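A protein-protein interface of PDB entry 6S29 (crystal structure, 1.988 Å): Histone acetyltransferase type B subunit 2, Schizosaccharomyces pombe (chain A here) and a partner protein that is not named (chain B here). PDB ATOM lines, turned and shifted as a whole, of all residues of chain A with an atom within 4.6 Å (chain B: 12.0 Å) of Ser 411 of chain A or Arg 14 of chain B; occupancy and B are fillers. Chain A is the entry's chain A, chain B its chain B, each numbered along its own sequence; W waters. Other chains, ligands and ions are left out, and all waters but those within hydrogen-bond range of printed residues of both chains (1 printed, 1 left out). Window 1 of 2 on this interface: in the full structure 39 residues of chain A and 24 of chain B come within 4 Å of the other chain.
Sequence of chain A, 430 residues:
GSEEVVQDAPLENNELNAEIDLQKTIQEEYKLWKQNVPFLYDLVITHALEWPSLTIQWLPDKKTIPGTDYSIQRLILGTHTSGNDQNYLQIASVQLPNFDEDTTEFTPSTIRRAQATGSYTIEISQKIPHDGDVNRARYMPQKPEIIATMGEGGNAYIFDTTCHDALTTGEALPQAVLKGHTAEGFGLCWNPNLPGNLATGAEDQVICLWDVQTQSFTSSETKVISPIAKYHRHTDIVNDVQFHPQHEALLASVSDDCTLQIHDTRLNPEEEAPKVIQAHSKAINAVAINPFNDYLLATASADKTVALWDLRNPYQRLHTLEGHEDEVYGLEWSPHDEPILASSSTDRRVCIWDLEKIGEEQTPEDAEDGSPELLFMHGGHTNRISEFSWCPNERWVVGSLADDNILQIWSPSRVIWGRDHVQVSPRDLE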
ATOM      1  N   TYR A  41      24.505  -4.912   2.487  1.00  0.00           N
ATOM      2  CA  TYR A  41      23.848  -3.647   2.203  1.00  0.00           C
ATOM      3  C   TYR A  41      24.722  -2.760   1.328  1.00  0.00           C
ATOM      4  O   TYR A  41      25.953  -2.858   1.343  1.00  0.00           O
ATOM      5  CB  TYR A  41      23.520  -2.874   3.496  1.00  0.00           C
ATOM      6  CG  TYR A  41      22.686  -3.624   4.504  1.00  0.00           C
ATOM      7  CD1 TYR A  41      23.279  -4.510   5.396  1.00  0.00           C
ATOM      8  CD2 TYR A  41      21.303  -3.417   4.592  1.00  0.00           C
ATOM      9  CE1 TYR A  41      22.525  -5.202   6.339  1.00  0.00           C
ATOM     10  CE2 TYR A  41      20.539  -4.095   5.546  1.00  0.00           C
ATOM     11  CZ  TYR A  41      21.169  -4.986   6.414  1.00  0.00           C
ATOM     12  OH  TYR A  41      20.449  -5.662   7.354  1.00  0.00           O
ATOM     13  N   ASP A  42      24.067  -1.894   0.557  1.00  0.00           N
ATOM     14  CA  ASP A  42      24.757  -0.760  -0.050  1.00  0.00           C
ATOM     15  C   ASP A  42      24.724   0.479   0.839  1.00  0.00           C
ATOM     16  O   ASP A  42      25.487   1.423   0.600  1.00  0.00           O
ATOM     17  CB  ASP A  42      24.145  -0.425  -1.415  1.00  0.00           C
ATOM     18  CG  ASP A  42      24.466  -1.461  -2.471  1.00  0.00           C
ATOM     19  OD1 ASP A  42      25.572  -2.046  -2.417  1.00  0.00           O
ATOM     20  OD2 ASP A  42      23.595  -1.694  -3.340  1.00  0.00           O
ATOM     21  N   LEU A  43      23.853   0.503   1.849  1.00  0.00           N
ATOM     22  CA  LEU A  43      23.736   1.657   2.736  1.00  0.00           C
ATOM     23  C   LEU A  43      23.164   1.201   4.070  1.00  0.00           C
ATOM     24  O   LEU A  43      22.160   0.480   4.101  1.00  0.00           O
ATOM     25  CB  LEU A  43      22.840   2.752   2.122  1.00  0.00           C
ATOM     26  CG  LEU A  43      22.567   4.011   2.973  1.00  0.00           C
ATOM     27  CD1 LEU A  43      23.737   4.969   2.980  1.00  0.00           C
ATOM     28  CD2 LEU A  43      21.308   4.742   2.494  1.00  0.00           C
ATOM     29  N   PHE A  99      24.155   8.109  -2.852  1.00  0.00           N
ATOM     30  CA  PHE A  99      24.862   6.839  -2.995  1.00  0.00           C
ATOM     31  C   PHE A  99      24.461   6.055  -4.234  1.00  0.00           C
ATOM     32  O   PHE A  99      24.977   4.953  -4.443  1.00  0.00           O
ATOM     33  CB  PHE A  99      24.662   5.970  -1.735  1.00  0.00           C
ATOM     34  CG  PHE A  99      23.335   5.228  -1.690  1.00  0.00           C
ATOM     35  CD1 PHE A  99      22.149   5.913  -1.474  1.00  0.00           C
ATOM     36  CD2 PHE A  99      23.285   3.845  -1.849  1.00  0.00           C
ATOM     37  CE1 PHE A  99      20.926   5.239  -1.422  1.00  0.00           C
ATOM     38  CE2 PHE A  99      22.076   3.168  -1.800  1.00  0.00           C
ATOM     39  CZ  PHE A  99      20.891   3.869  -1.587  1.00  0.00           C
ATOM     40  N   ASP A 100      23.613   6.614  -5.094  1.00  0.00           N
ATOM     41  CA  ASP A 100      22.970   5.857  -6.169  1.00  0.00           C
ATOM     42  C   ASP A 100      22.950   6.714  -7.427  1.00  0.00           C
ATOM     43  O   ASP A 100      22.233   7.720  -7.475  1.00  0.00           O
ATOM     44  CB  ASP A 100      21.545   5.456  -5.762  1.00  0.00           C
ATOM     45  CG  ASP A 100      20.943   4.392  -6.666  1.00  0.00           C
ATOM     46  OD1 ASP A 100      21.386   4.252  -7.826  1.00  0.00           O
ATOM     47  OD2 ASP A 100      20.002   3.701  -6.214  1.00  0.00           O
ATOM     48  N   GLU A 101      23.709   6.296  -8.452  1.00  0.00           N
ATOM     49  CA  GLU A 101      23.742   7.030  -9.719  1.00  0.00           C
ATOM     50  C   GLU A 101      22.346   7.216 -10.305  1.00  0.00           C
ATOM     51  O   GLU A 101      22.091   8.199 -11.011  1.00  0.00           O
ATOM     52  CB  GLU A 101      24.656   6.312 -10.718  1.00  0.00           C
ATOM     53  CG  GLU A 101      24.945   7.083 -12.007  1.00  0.00           C
ATOM     54  CD  GLU A 101      25.992   8.190 -11.836  1.00  0.00           C
ATOM     55  OE1 GLU A 101      25.782   9.294 -12.386  1.00  0.00           O
ATOM     56  OE2 GLU A 101      27.023   7.965 -11.162  1.00  0.00           O
ATOM     57  N   ARG A 395      15.985   3.791  -4.312  1.00  0.00           N
ATOM     58  CA  ARG A 395      15.869   2.405  -4.742  1.00  0.00           C
ATOM     59  C   ARG A 395      16.150   1.497  -3.546  1.00  0.00           C
ATOM     60  O   ARG A 395      17.267   1.479  -3.018  1.00  0.00           O
ATOM     61  CB  ARG A 395      16.827   2.129  -5.897  1.00  0.00           C
ATOM     62  CG  ARG A 395      16.410   2.826  -7.205  1.00  0.00           C
ATOM     63  CD  ARG A 395      17.139   2.225  -8.408  1.00  0.00           C
ATOM     64  NE  ARG A 395      18.591   2.395  -8.315  1.00  0.00           N
ATOM     65  CZ  ARG A 395      19.469   1.834  -9.141  1.00  0.00           C
ATOM     66  NH1 ARG A 395      19.045   1.064 -10.136  1.00  0.00           N
ATOM     67  NH2 ARG A 395      20.772   2.058  -8.982  1.00  0.00           N
ATOM     68  N   TRP A 396      15.116   0.780  -3.098  1.00  0.00           N
ATOM     69  CA  TRP A 396      15.232  -0.256  -2.071  1.00  0.00           C
ATOM     70  C   TRP A 396      15.800   0.307  -0.764  1.00  0.00           C
ATOM     71  O   TRP A 396      16.688  -0.276  -0.146  1.00  0.00           O
ATOM     72  CB  TRP A 396      16.075  -1.438  -2.575  1.00  0.00           C
ATOM     73  CG  TRP A 396      15.379  -2.235  -3.670  1.00  0.00           C
ATOM     74  CD1 TRP A 396      15.168  -1.835  -4.965  1.00  0.00           C
ATOM     75  CD2 TRP A 396      14.804  -3.547  -3.559  1.00  0.00           C
ATOM     76  NE1 TRP A 396      14.501  -2.814  -5.663  1.00  0.00           N
ATOM     77  CE2 TRP A 396      14.263  -3.874  -4.827  1.00  0.00           C
ATOM     78  CE3 TRP A 396      14.695  -4.479  -2.519  1.00  0.00           C
ATOM     79  CZ2 TRP A 396      13.618  -5.090  -5.079  1.00  0.00           C
ATOM     80  CZ3 TRP A 396      14.045  -5.696  -2.774  1.00  0.00           C
ATOM     81  CH2 TRP A 396      13.519  -5.985  -4.047  1.00  0.00           C
ATOM     82  N   VAL A 397      15.268   1.445  -0.321  1.00  0.00           N
ATOM     83  CA  VAL A 397      15.689   2.048   0.942  1.00  0.00           C
ATOM     84  C   VAL A 397      14.513   2.002   1.910  1.00  0.00           C
ATOM     85  O   VAL A 397      13.392   2.399   1.559  1.00  0.00           O
ATOM     86  CB  VAL A 397      16.187   3.491   0.744  1.00  0.00           C
ATOM     87  CG1 VAL A 397      16.332   4.202   2.095  1.00  0.00           C
ATOM     88  CG2 VAL A 397      17.498   3.504  -0.007  1.00  0.00           C
ATOM     89  N   TRP A 410      18.310   1.852   5.715  1.00  0.00           N
ATOM     90  CA  TRP A 410      19.132   0.809   5.115  1.00  0.00           C
ATOM     91  C   TRP A 410      18.645   0.438   3.723  1.00  0.00           C
ATOM     92  O   TRP A 410      17.484   0.654   3.354  1.00  0.00           O
ATOM     93  CB  TRP A 410      19.202  -0.451   5.994  1.00  0.00           C
ATOM     94  CG  TRP A 410      17.881  -0.915   6.527  1.00  0.00           C
ATOM     95  CD1 TRP A 410      17.284  -0.520   7.689  1.00  0.00           C
ATOM     96  CD2 TRP A 410      16.998  -1.878   5.929  1.00  0.00           C
ATOM     97  NE1 TRP A 410      16.070  -1.157   7.847  1.00  0.00           N
ATOM     98  CE2 TRP A 410      15.873  -2.006   6.790  1.00  0.00           C
ATOM     99  CE3 TRP A 410      17.041  -2.633   4.753  1.00  0.00           C
ATOM    100  CZ2 TRP A 410      14.803  -2.880   6.518  1.00  0.00           C
ATOM    101  CZ3 TRP A 410      15.970  -3.501   4.478  1.00  0.00           C
ATOM    102  CH2 TRP A 410      14.866  -3.616   5.365  1.00  0.00           C
ATOM    103  N   SER A 411      19.558  -0.169   2.964  1.00  0.00           N
ATOM    104  CA  SER A 411      19.275  -0.536   1.589  1.00  0.00           C
ATOM    105  C   SER A 411      20.064  -1.800   1.283  1.00  0.00           C
ATOM    106  O   SER A 411      21.299  -1.780   1.326  1.00  0.00           O
ATOM    107  CB  SER A 411      19.672   0.616   0.649  1.00  0.00           C
ATOM    108  OG  SER A 411      19.238   0.406  -0.685  1.00  0.00           O
ATOM    109  N   PRO A 412      19.394  -2.908   0.954  1.00  0.00           N
ATOM    110  CA  PRO A 412      20.121  -4.142   0.612  1.00  0.00           C
ATOM    111  C   PRO A 412      20.971  -3.979  -0.645  1.00  0.00           C
ATOM    112  O   PRO A 412      20.670  -3.177  -1.524  1.00  0.00           O
ATOM    113  CB  PRO A 412      18.997  -5.164   0.380  1.00  0.00           C
ATOM    114  CG  PRO A 412      17.779  -4.310   0.034  1.00  0.00           C
ATOM    115  CD  PRO A 412      17.929  -3.090   0.900  1.00  0.00           C
ATOM    116  N   SER A 413      22.039  -4.769  -0.724  1.00  0.00           N
ATOM    117  CA  SER A 413      22.927  -4.723  -1.880  1.00  0.00           C
ATOM    118  C   SER A 413      22.173  -4.976  -3.185  1.00  0.00           C
ATOM    119  O   SER A 413      21.365  -5.907  -3.286  1.00  0.00           O
ATOM    120  CB  SER A 413      24.055  -5.732  -1.722  1.00  0.00           C
ATOM    121  OG  SER A 413      24.731  -5.918  -2.949  1.00  0.00           O
ATOM    122  N   ARG A 414      22.450  -4.129  -4.193  1.00  0.00           N
ATOM    123  CA  ARG A 414      21.872  -4.307  -5.526  1.00  0.00           C
ATOM    124  C   ARG A 414      22.229  -5.655  -6.137  1.00  0.00           C
ATOM    125  O   ARG A 414      21.494  -6.157  -6.992  1.00  0.00           O
ATOM    126  CB  ARG A 414      22.339  -3.189  -6.461  1.00  0.00           C
ATOM    127  CG  ARG A 414      21.592  -3.167  -7.819  1.00  0.00           C
ATOM    128  CD  ARG A 414      22.055  -2.034  -8.756  1.00  0.00           C
ATOM    129  NE  ARG A 414      23.511  -1.860  -8.746  1.00  0.00           N
ATOM    130  CZ  ARG A 414      24.158  -0.893  -9.394  1.00  0.00           C
ATOM    131  NH1 ARG A 414      23.487  -0.002 -10.110  1.00  0.00           N
ATOM    132  NH2 ARG A 414      25.478  -0.812  -9.321  1.00  0.00           N
ATOM    133  N   TRP A 417      19.083  -7.797  -5.228  1.00  0.00           N
ATOM    134  CA  TRP A 417      17.756  -7.565  -5.787  1.00  0.00           C
ATOM    135  C   TRP A 417      17.756  -7.207  -7.265  1.00  0.00           C
ATOM    136  O   TRP A 417      16.683  -7.210  -7.878  1.00  0.00           O
ATOM    137  CB  TRP A 417      17.020  -6.468  -4.997  1.00  0.00           C
ATOM    138  CG  TRP A 417      17.769  -5.152  -4.859  1.00  0.00           C
ATOM    139  CD1 TRP A 417      18.542  -4.753  -3.808  1.00  0.00           C
ATOM    140  CD2 TRP A 417      17.778  -4.072  -5.799  1.00  0.00           C
ATOM    141  NE1 TRP A 417      19.028  -3.484  -4.029  1.00  0.00           N
ATOM    142  CE2 TRP A 417      18.577  -3.046  -5.249  1.00  0.00           C
ATOM    143  CE3 TRP A 417      17.183  -3.871  -7.053  1.00  0.00           C
ATOM    144  CZ2 TRP A 417      18.818  -1.851  -5.917  1.00  0.00           C
ATOM    145  CZ3 TRP A 417      17.416  -2.676  -7.712  1.00  0.00           C
ATOM    146  CH2 TRP A 417      18.224  -1.679  -7.140  1.00  0.00           C
ATOM    147  N   GLU B   7      25.609   7.506  12.625  1.00  0.00           N
ATOM    148  CA  GLU B   7      26.653   6.544  12.280  1.00  0.00           C
ATOM    149  C   GLU B   7      26.371   5.950  10.897  1.00  0.00           C
ATOM    150  O   GLU B   7      25.297   5.384  10.659  1.00  0.00           O
ATOM    151  CB  GLU B   7      26.726   5.415  13.306  1.00  0.00           C
ATOM    152  CG  GLU B   7      27.027   5.838  14.732  1.00  0.00           C
ATOM    153  CD  GLU B   7      27.439   4.656  15.597  1.00  0.00           C
ATOM    154  OE1 GLU B   7      26.887   4.502  16.712  1.00  0.00           O
ATOM    155  OE2 GLU B   7      28.309   3.871  15.147  1.00  0.00           O
ATOM    156  N   LEU B   8      27.361   6.035  10.005  1.00  0.00           N
ATOM    157  CA  LEU B   8      27.288   5.433   8.671  1.00  0.00           C
ATOM    158  C   LEU B   8      28.096   4.143   8.682  1.00  0.00           C
ATOM    159  O   LEU B   8      29.328   4.172   8.630  1.00  0.00           O
ATOM    160  CB  LEU B   8      27.801   6.401   7.610  1.00  0.00           C
ATOM    161  CG  LEU B   8      27.802   5.896   6.164  1.00  0.00           C
ATOM    162  CD1 LEU B   8      26.372   5.830   5.607  1.00  0.00           C
ATOM    163  CD2 LEU B   8      28.707   6.754   5.279  1.00  0.00           C
ATOM    164  N   LEU B   9      27.396   3.009   8.737  1.00  0.00           N
ATOM    165  CA  LEU B   9      28.071   1.721   8.866  1.00  0.00           C
ATOM    166  C   LEU B   9      28.605   1.206   7.538  1.00  0.00           C
ATOM    167  O   LEU B   9      29.556   0.420   7.530  1.00  0.00           O
ATOM    168  CB  LEU B   9      27.123   0.691   9.478  1.00  0.00           C
ATOM    169  CG  LEU B   9      26.665   0.957  10.910  1.00  0.00           C
ATOM    170  CD1 LEU B   9      25.957  -0.277  11.486  1.00  0.00           C
ATOM    171  CD2 LEU B   9      27.854   1.338  11.767  1.00  0.00           C
ATOM    172  N   VAL B  10      27.981   1.570   6.421  1.00  0.00           N
ATOM    173  CA  VAL B  10      28.455   1.140   5.113  1.00  0.00           C
ATOM    174  C   VAL B  10      27.855   2.046   4.047  1.00  0.00           C
ATOM    175  O   VAL B  10      26.698   2.480   4.146  1.00  0.00           O
ATOM    176  CB  VAL B  10      28.127  -0.352   4.848  1.00  0.00           C
ATOM    177  CG1 VAL B  10      26.621  -0.581   4.656  1.00  0.00           C
ATOM    178  CG2 VAL B  10      28.928  -0.873   3.646  1.00  0.00           C
ATOM    179  N   LEU B  11      28.668   2.340   3.032  1.00  0.00           N
ATOM    180  CA  LEU B  11      28.215   3.034   1.833  1.00  0.00           C
ATOM    181  C   LEU B  11      28.971   2.465   0.642  1.00  0.00           C
ATOM    182  O   LEU B  11      30.198   2.570   0.580  1.00  0.00           O
ATOM    183  CB  LEU B  11      28.443   4.544   1.943  1.00  0.00           C
ATOM    184  CG  LEU B  11      27.655   5.436   0.974  1.00  0.00           C
ATOM    185  CD1 LEU B  11      27.523   6.818   1.561  1.00  0.00           C
ATOM    186  CD2 LEU B  11      28.268   5.514  -0.427  1.00  0.00           C
ATOM    187  N   ARG B  12      28.244   1.884  -0.306  1.00  0.00           N
ATOM    188  CA  ARG B  12      28.833   1.405  -1.549  1.00  0.00           C
ATOM    189  C   ARG B  12      28.051   2.038  -2.691  1.00  0.00           C
ATOM    190  O   ARG B  12      26.858   1.751  -2.874  1.00  0.00           O
ATOM    191  CB  ARG B  12      28.830  -0.124  -1.648  1.00  0.00           C
ATOM    192  CG  ARG B  12      29.802  -0.637  -2.730  1.00  0.00           C
ATOM    193  CD  ARG B  12      31.148   0.157  -2.707  1.00  0.00           C
ATOM    194  NE  ARG B  12      31.348   1.048  -3.861  1.00  0.00           N
ATOM    195  CZ  ARG B  12      31.974   2.227  -3.815  1.00  0.00           C
ATOM    196  NH1 ARG B  12      32.442   2.696  -2.660  1.00  0.00           N
ATOM    197  NH2 ARG B  12      32.106   2.955  -4.924  1.00  0.00           N
ATOM    198  N   PHE B  13      28.716   2.931  -3.419  1.00  0.00           N
ATOM    199  CA  PHE B  13      28.068   3.668  -4.491  1.00  0.00           C
ATOM    200  C   PHE B  13      27.623   2.727  -5.608  1.00  0.00           C
ATOM    201  O   PHE B  13      28.366   1.835  -6.025  1.00  0.00           O
ATOM    202  CB  PHE B  13      29.022   4.744  -5.032  1.00  0.00           C
ATOM    203  CG  PHE B  13      28.356   5.689  -5.981  1.00  0.00           C
ATOM    204  CD1 PHE B  13      27.550   6.709  -5.504  1.00  0.00           C
ATOM    205  CD2 PHE B  13      28.505   5.539  -7.344  1.00  0.00           C
ATOM    206  CE1 PHE B  13      26.893   7.541  -6.370  1.00  0.00           C
ATOM    207  CE2 PHE B  13      27.880   6.393  -8.223  1.00  0.00           C
ATOM    208  CZ  PHE B  13      27.068   7.388  -7.745  1.00  0.00           C
ATOM    209  N   ARG B  14      26.395   2.930  -6.090  1.00  0.00           N
ATOM    210  CA  ARG B  14      25.839   2.144  -7.192  1.00  0.00           C
ATOM    211  C   ARG B  14      26.200   2.860  -8.488  1.00  0.00           C
ATOM    212  O   ARG B  14      25.615   3.896  -8.823  1.00  0.00           O
ATOM    213  CB  ARG B  14      24.329   1.973  -7.048  1.00  0.00           C
ATOM    214  CG  ARG B  14      23.922   1.154  -5.819  1.00  0.00           C
ATOM    215  CD  ARG B  14      22.435   1.286  -5.483  1.00  0.00           C
ATOM    216  NE  ARG B  14      22.048   0.354  -4.423  1.00  0.00           N
ATOM    217  CZ  ARG B  14      20.885   0.393  -3.776  1.00  0.00           C
ATOM    218  NH1 ARG B  14      19.984   1.319  -4.089  1.00  0.00           N
ATOM    219  NH2 ARG B  14      20.611  -0.504  -2.830  1.00  0.00           N
ATOM    220  N   GLU B  15      27.186   2.323  -9.209  1.00  0.00           N
ATOM    221  CA  GLU B  15      27.582   2.900 -10.486  1.00  0.00           C
ATOM    222  C   GLU B  15      26.478   2.745 -11.528  1.00  0.00           C
ATOM    223  O   GLU B  15      25.530   1.974 -11.366  1.00  0.00           O
ATOM    224  CB  GLU B  15      28.886   2.271 -10.993  1.00  0.00           C
ATOM    225  CG  GLU B  15      30.134   2.725 -10.233  1.00  0.00           C
ATOM    226  CD  GLU B  15      30.447   4.199 -10.447  1.00  0.00           C
ATOM    227  OE1 GLU B  15      29.967   4.773 -11.450  1.00  0.00           O
ATOM    228  OE2 GLU B  15      31.166   4.789  -9.610  1.00  0.00           O
ATOM    229  N   PHE B  16      26.620   3.524 -12.602  1.00  0.00           N
ATOM    230  CA  PHE B  16      25.683   3.540 -13.722  1.00  0.00           C
ATOM    231  C   PHE B  16      25.405   2.138 -14.252  1.00  0.00           C
ATOM    232  O   PHE B  16      26.322   1.342 -14.469  1.00  0.00           O
ATOM    233  CB  PHE B  16      26.258   4.422 -14.839  1.00  0.00           C
ATOM    234  CG  PHE B  16      25.272   4.824 -15.933  1.00  0.00           C
ATOM    235  CD1 PHE B  16      25.577   5.891 -16.767  1.00  0.00           C
ATOM    236  CD2 PHE B  16      24.076   4.148 -16.152  1.00  0.00           C
ATOM    237  CE1 PHE B  16      24.711   6.278 -17.784  1.00  0.00           C
ATOM    238  CE2 PHE B  16      23.211   4.523 -17.163  1.00  0.00           C
ATOM    239  CZ  PHE B  16      23.527   5.593 -17.981  1.00  0.00           C
ATOM    240  N   GLY B  17      24.116   1.848 -14.437  1.00  0.00           N
ATOM    241  CA  GLY B  17      23.642   0.752 -15.259  1.00  0.00           C
ATOM    242  C   GLY B  17      23.351  -0.545 -14.543  1.00  0.00           C
ATOM    243  O   GLY B  17      24.140  -0.998 -13.709  1.00  0.00           O
ATOM    244  N   VAL B  18      22.212  -1.150 -14.883  1.00  0.00           N
ATOM    245  CA  VAL B  18      21.793  -2.454 -14.356  1.00  0.00           C
ATOM    246  C   VAL B  18      21.097  -3.200 -15.495  1.00  0.00           C
ATOM    247  O   VAL B  18      20.246  -2.636 -16.192  1.00  0.00           O
ATOM    248  CB  VAL B  18      20.847  -2.352 -13.106  1.00  0.00           C
ATOM    249  CG1 VAL B  18      20.850  -3.671 -12.309  1.00  0.00           C
ATOM    250  CG2 VAL B  18      21.191  -1.159 -12.196  1.00  0.00           C
HETATM  251  O   HOH W   1      28.535   0.012  -8.647  1.00  0.00           O
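Water W1 lies within hydrogen-bond range of the backbone NH (N) of Glu 15 of chain B (2.7 Å), the backbone carbonyl oxygen (O) of Phe 13 of chain B (3.2 Å) and the guanidinium group (NH2) of Arg 414 of chain A (3.2 Å).
The side-chain carboxylate (OD2) of Asp 42 of chain A sits at hydrogen-bond distance from the backbone NH (N) of Arg 414 of chain A, at 2.8 Å.
The backbone carbonyl oxygen (O) of Leu 43 of chain A lies within hydrogen-bond range of the backbone NH (N) of Ser 411 of chain A (2.9 Å).
The indole nitrogen of Trp 417 of chain A sits at hydrogen-bond distance from the backbone carbonyl oxygen of Pro 412 of chain A (3.0 Å).
The backbone carbonyl oxygen of Ser 413 of chain A lies close to the indole nitrogen of Trp 417 of chain A.
N of Asp 42 of chain A sits at hydrogen-bond distance from O of Ser 411 of chain A (2.9 Å).
OG of Ser 411 of chain A is in hydrogen-bond range of O of Trp 396 of chain A (2.7 Å).
The backbone carbonyl oxygen (O) of Pro 412 of chain A sits at hydrogen-bond distance from the guanidinium group (NH2) of Arg 14 of chain B, 3.0 Å away.
The backbone carbonyl oxygen of Phe 99 of chain A lies within hydrogen-bond range of the backbone NH of Arg 14 of chain B, at 3.0 Å.
OD2 of Asp 42 of chain A is in salt-bridge range of NE of Arg 14 of chain B.
The guanidinium group (NH2) of Arg 14 of chain B sits at hydrogen-bond distance from the side-chain hydroxyl (OG) of Ser 411 of chain A, at 2.7 Å.
The guanidinium group (NH1) of Arg 14 of chain B lies within salt-bridge range of the side-chain carboxylate (OD2) of Asp 100 of chain A (3.2 Å).
NH1 of Arg 414 of chain A is in hydrogen-bond range of O of Glu 15 of chain B (3.1 Å).
The backbone carbonyl oxygen of Asp 42 of chain A lies within hydrogen-bond range of the backbone NH of Arg 12 of chain B.
The backbone NH (N) of Glu 101 of chain A is in hydrogen-bond range of the backbone carbonyl oxygen (O) of Arg 14 of chain B (3.1 Å).
O of Arg 395 of chain A is in hydrogen-bond range of NH1 of Arg 14 of chain B, at 2.9 Å.
Among the printed residues, pairs that only touch across the chains: Asp 42 of chain A with Val 10 of chain B (3.9 Å), Asp 42 of chain A with Leu 11 of chain B (3.4 Å), Leu 43 of chain A with Leu 8 of chain B (3.8 Å), Leu 43 of chain A with Val 10 of chain B (3.4 Å), Phe 99 of chain A with Leu 11 of chain B (3.9 Å), Phe 99 of chain A with Phe 13 of chain B (3.3 Å), Asp 100 of chain A with Phe 13 of chain B (3.6 Å), Glu 101 of chain A with Phe 13 of chain B (3.4 Å), Glu 101 of chain A with Phe 16 of chain B (3.9 Å), Arg 395 of chain A with Val 18 of chain B (3.7 Å), Arg 414 of chain A with Arg 14 of chain B (3.7 Å), Arg 414 of chain A with Gly 17 of chain B (3.8 Å), Arg 414 of chain A with Val 18 of chain B (3.3 Å) and Trp 417 of chain A with Arg 14 of chain B (3.6 Å).
Of the printed residues of chain B, Ser 411 of chain A touches Arg 14.
Of chain A, only Asp 42 (2.8 Å), Phe 99 (3.0 Å), Asp 100 (3.2 Å), Glu 101 (3.1 Å), Arg 395 (2.9 Å), Ser 411 (2.7 Å), Pro 412 (3.0 Å), Arg 414 (3.7 Å) and Trp 417 (3.6 Å) come within 4 Å of Arg 14 of chain B.
No residue of chain B comes within 4 Å of Tyr 41 of chain A.
Asp 42 of chain A touches four residues of chain B.
Of chain B, only Leu 11, Phe 13 and Arg 14 come within 4 Å of Phe 99 of chain A.
Of chain B, only Phe 13 (3.6 Å) and Arg 14 (3.2 Å) come within 4 Å of Asp 100 of chain A.
Of chain B, only Arg 14 (2.9 Å) and Val 18 (3.7 Å) come within 4 Å of Arg 395 of chain A.
No residue of chain B comes within 4 Å of Val 397 of chain A.
No residue of chain B comes within 4 Å of Trp 410 of chain A.
Of chain B, only Arg 14 comes within 4 Å of Pro 412 of chain A.
Ser 413 of chain A touches none of the printed residues of chain B.
Of the printed residues of chain A, Leu 8 of chain B touches Leu 43 (3.8 Å).
Of the printed residues of chain A, Phe 13 of chain B touches Phe 99, Asp 100 and Glu 101.
Of the printed residues of chain A, Val 18 of chain B touches Arg 395 and Arg 414.
Of the printed residues of chain A, Gly 17 of chain B touches Arg 414 (3.8 Å).
Trp 396 of chain A touches none of the printed residues of chain B.
Leu 9 of chain B touches none of the printed residues of chain A.
The nearest printed residue of chain A that does not touch Arg 14 of chain B is Trp 396 of chain A (4.6 Å).
The nearest printed residue of chain A that does not touch Leu 8 of chain B is Asp 42 of chain A (6.7 Å).
Of the 15 printed residues of chain A, 10 touch a printed residue of chain B.
Printed residues of chain B that touch a printed residue of chain A: Leu 8, Val 10, Leu 11, Arg 12, Phe 13, Arg 14, Glu 15, Phe 16, Gly 17 and Val 18.
Hydrophobic or aromatic side chains of chain B within 4 Å of the printed part of chain A: Leu 8, Val 10, Leu 11, Phe 13 and Val 18.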
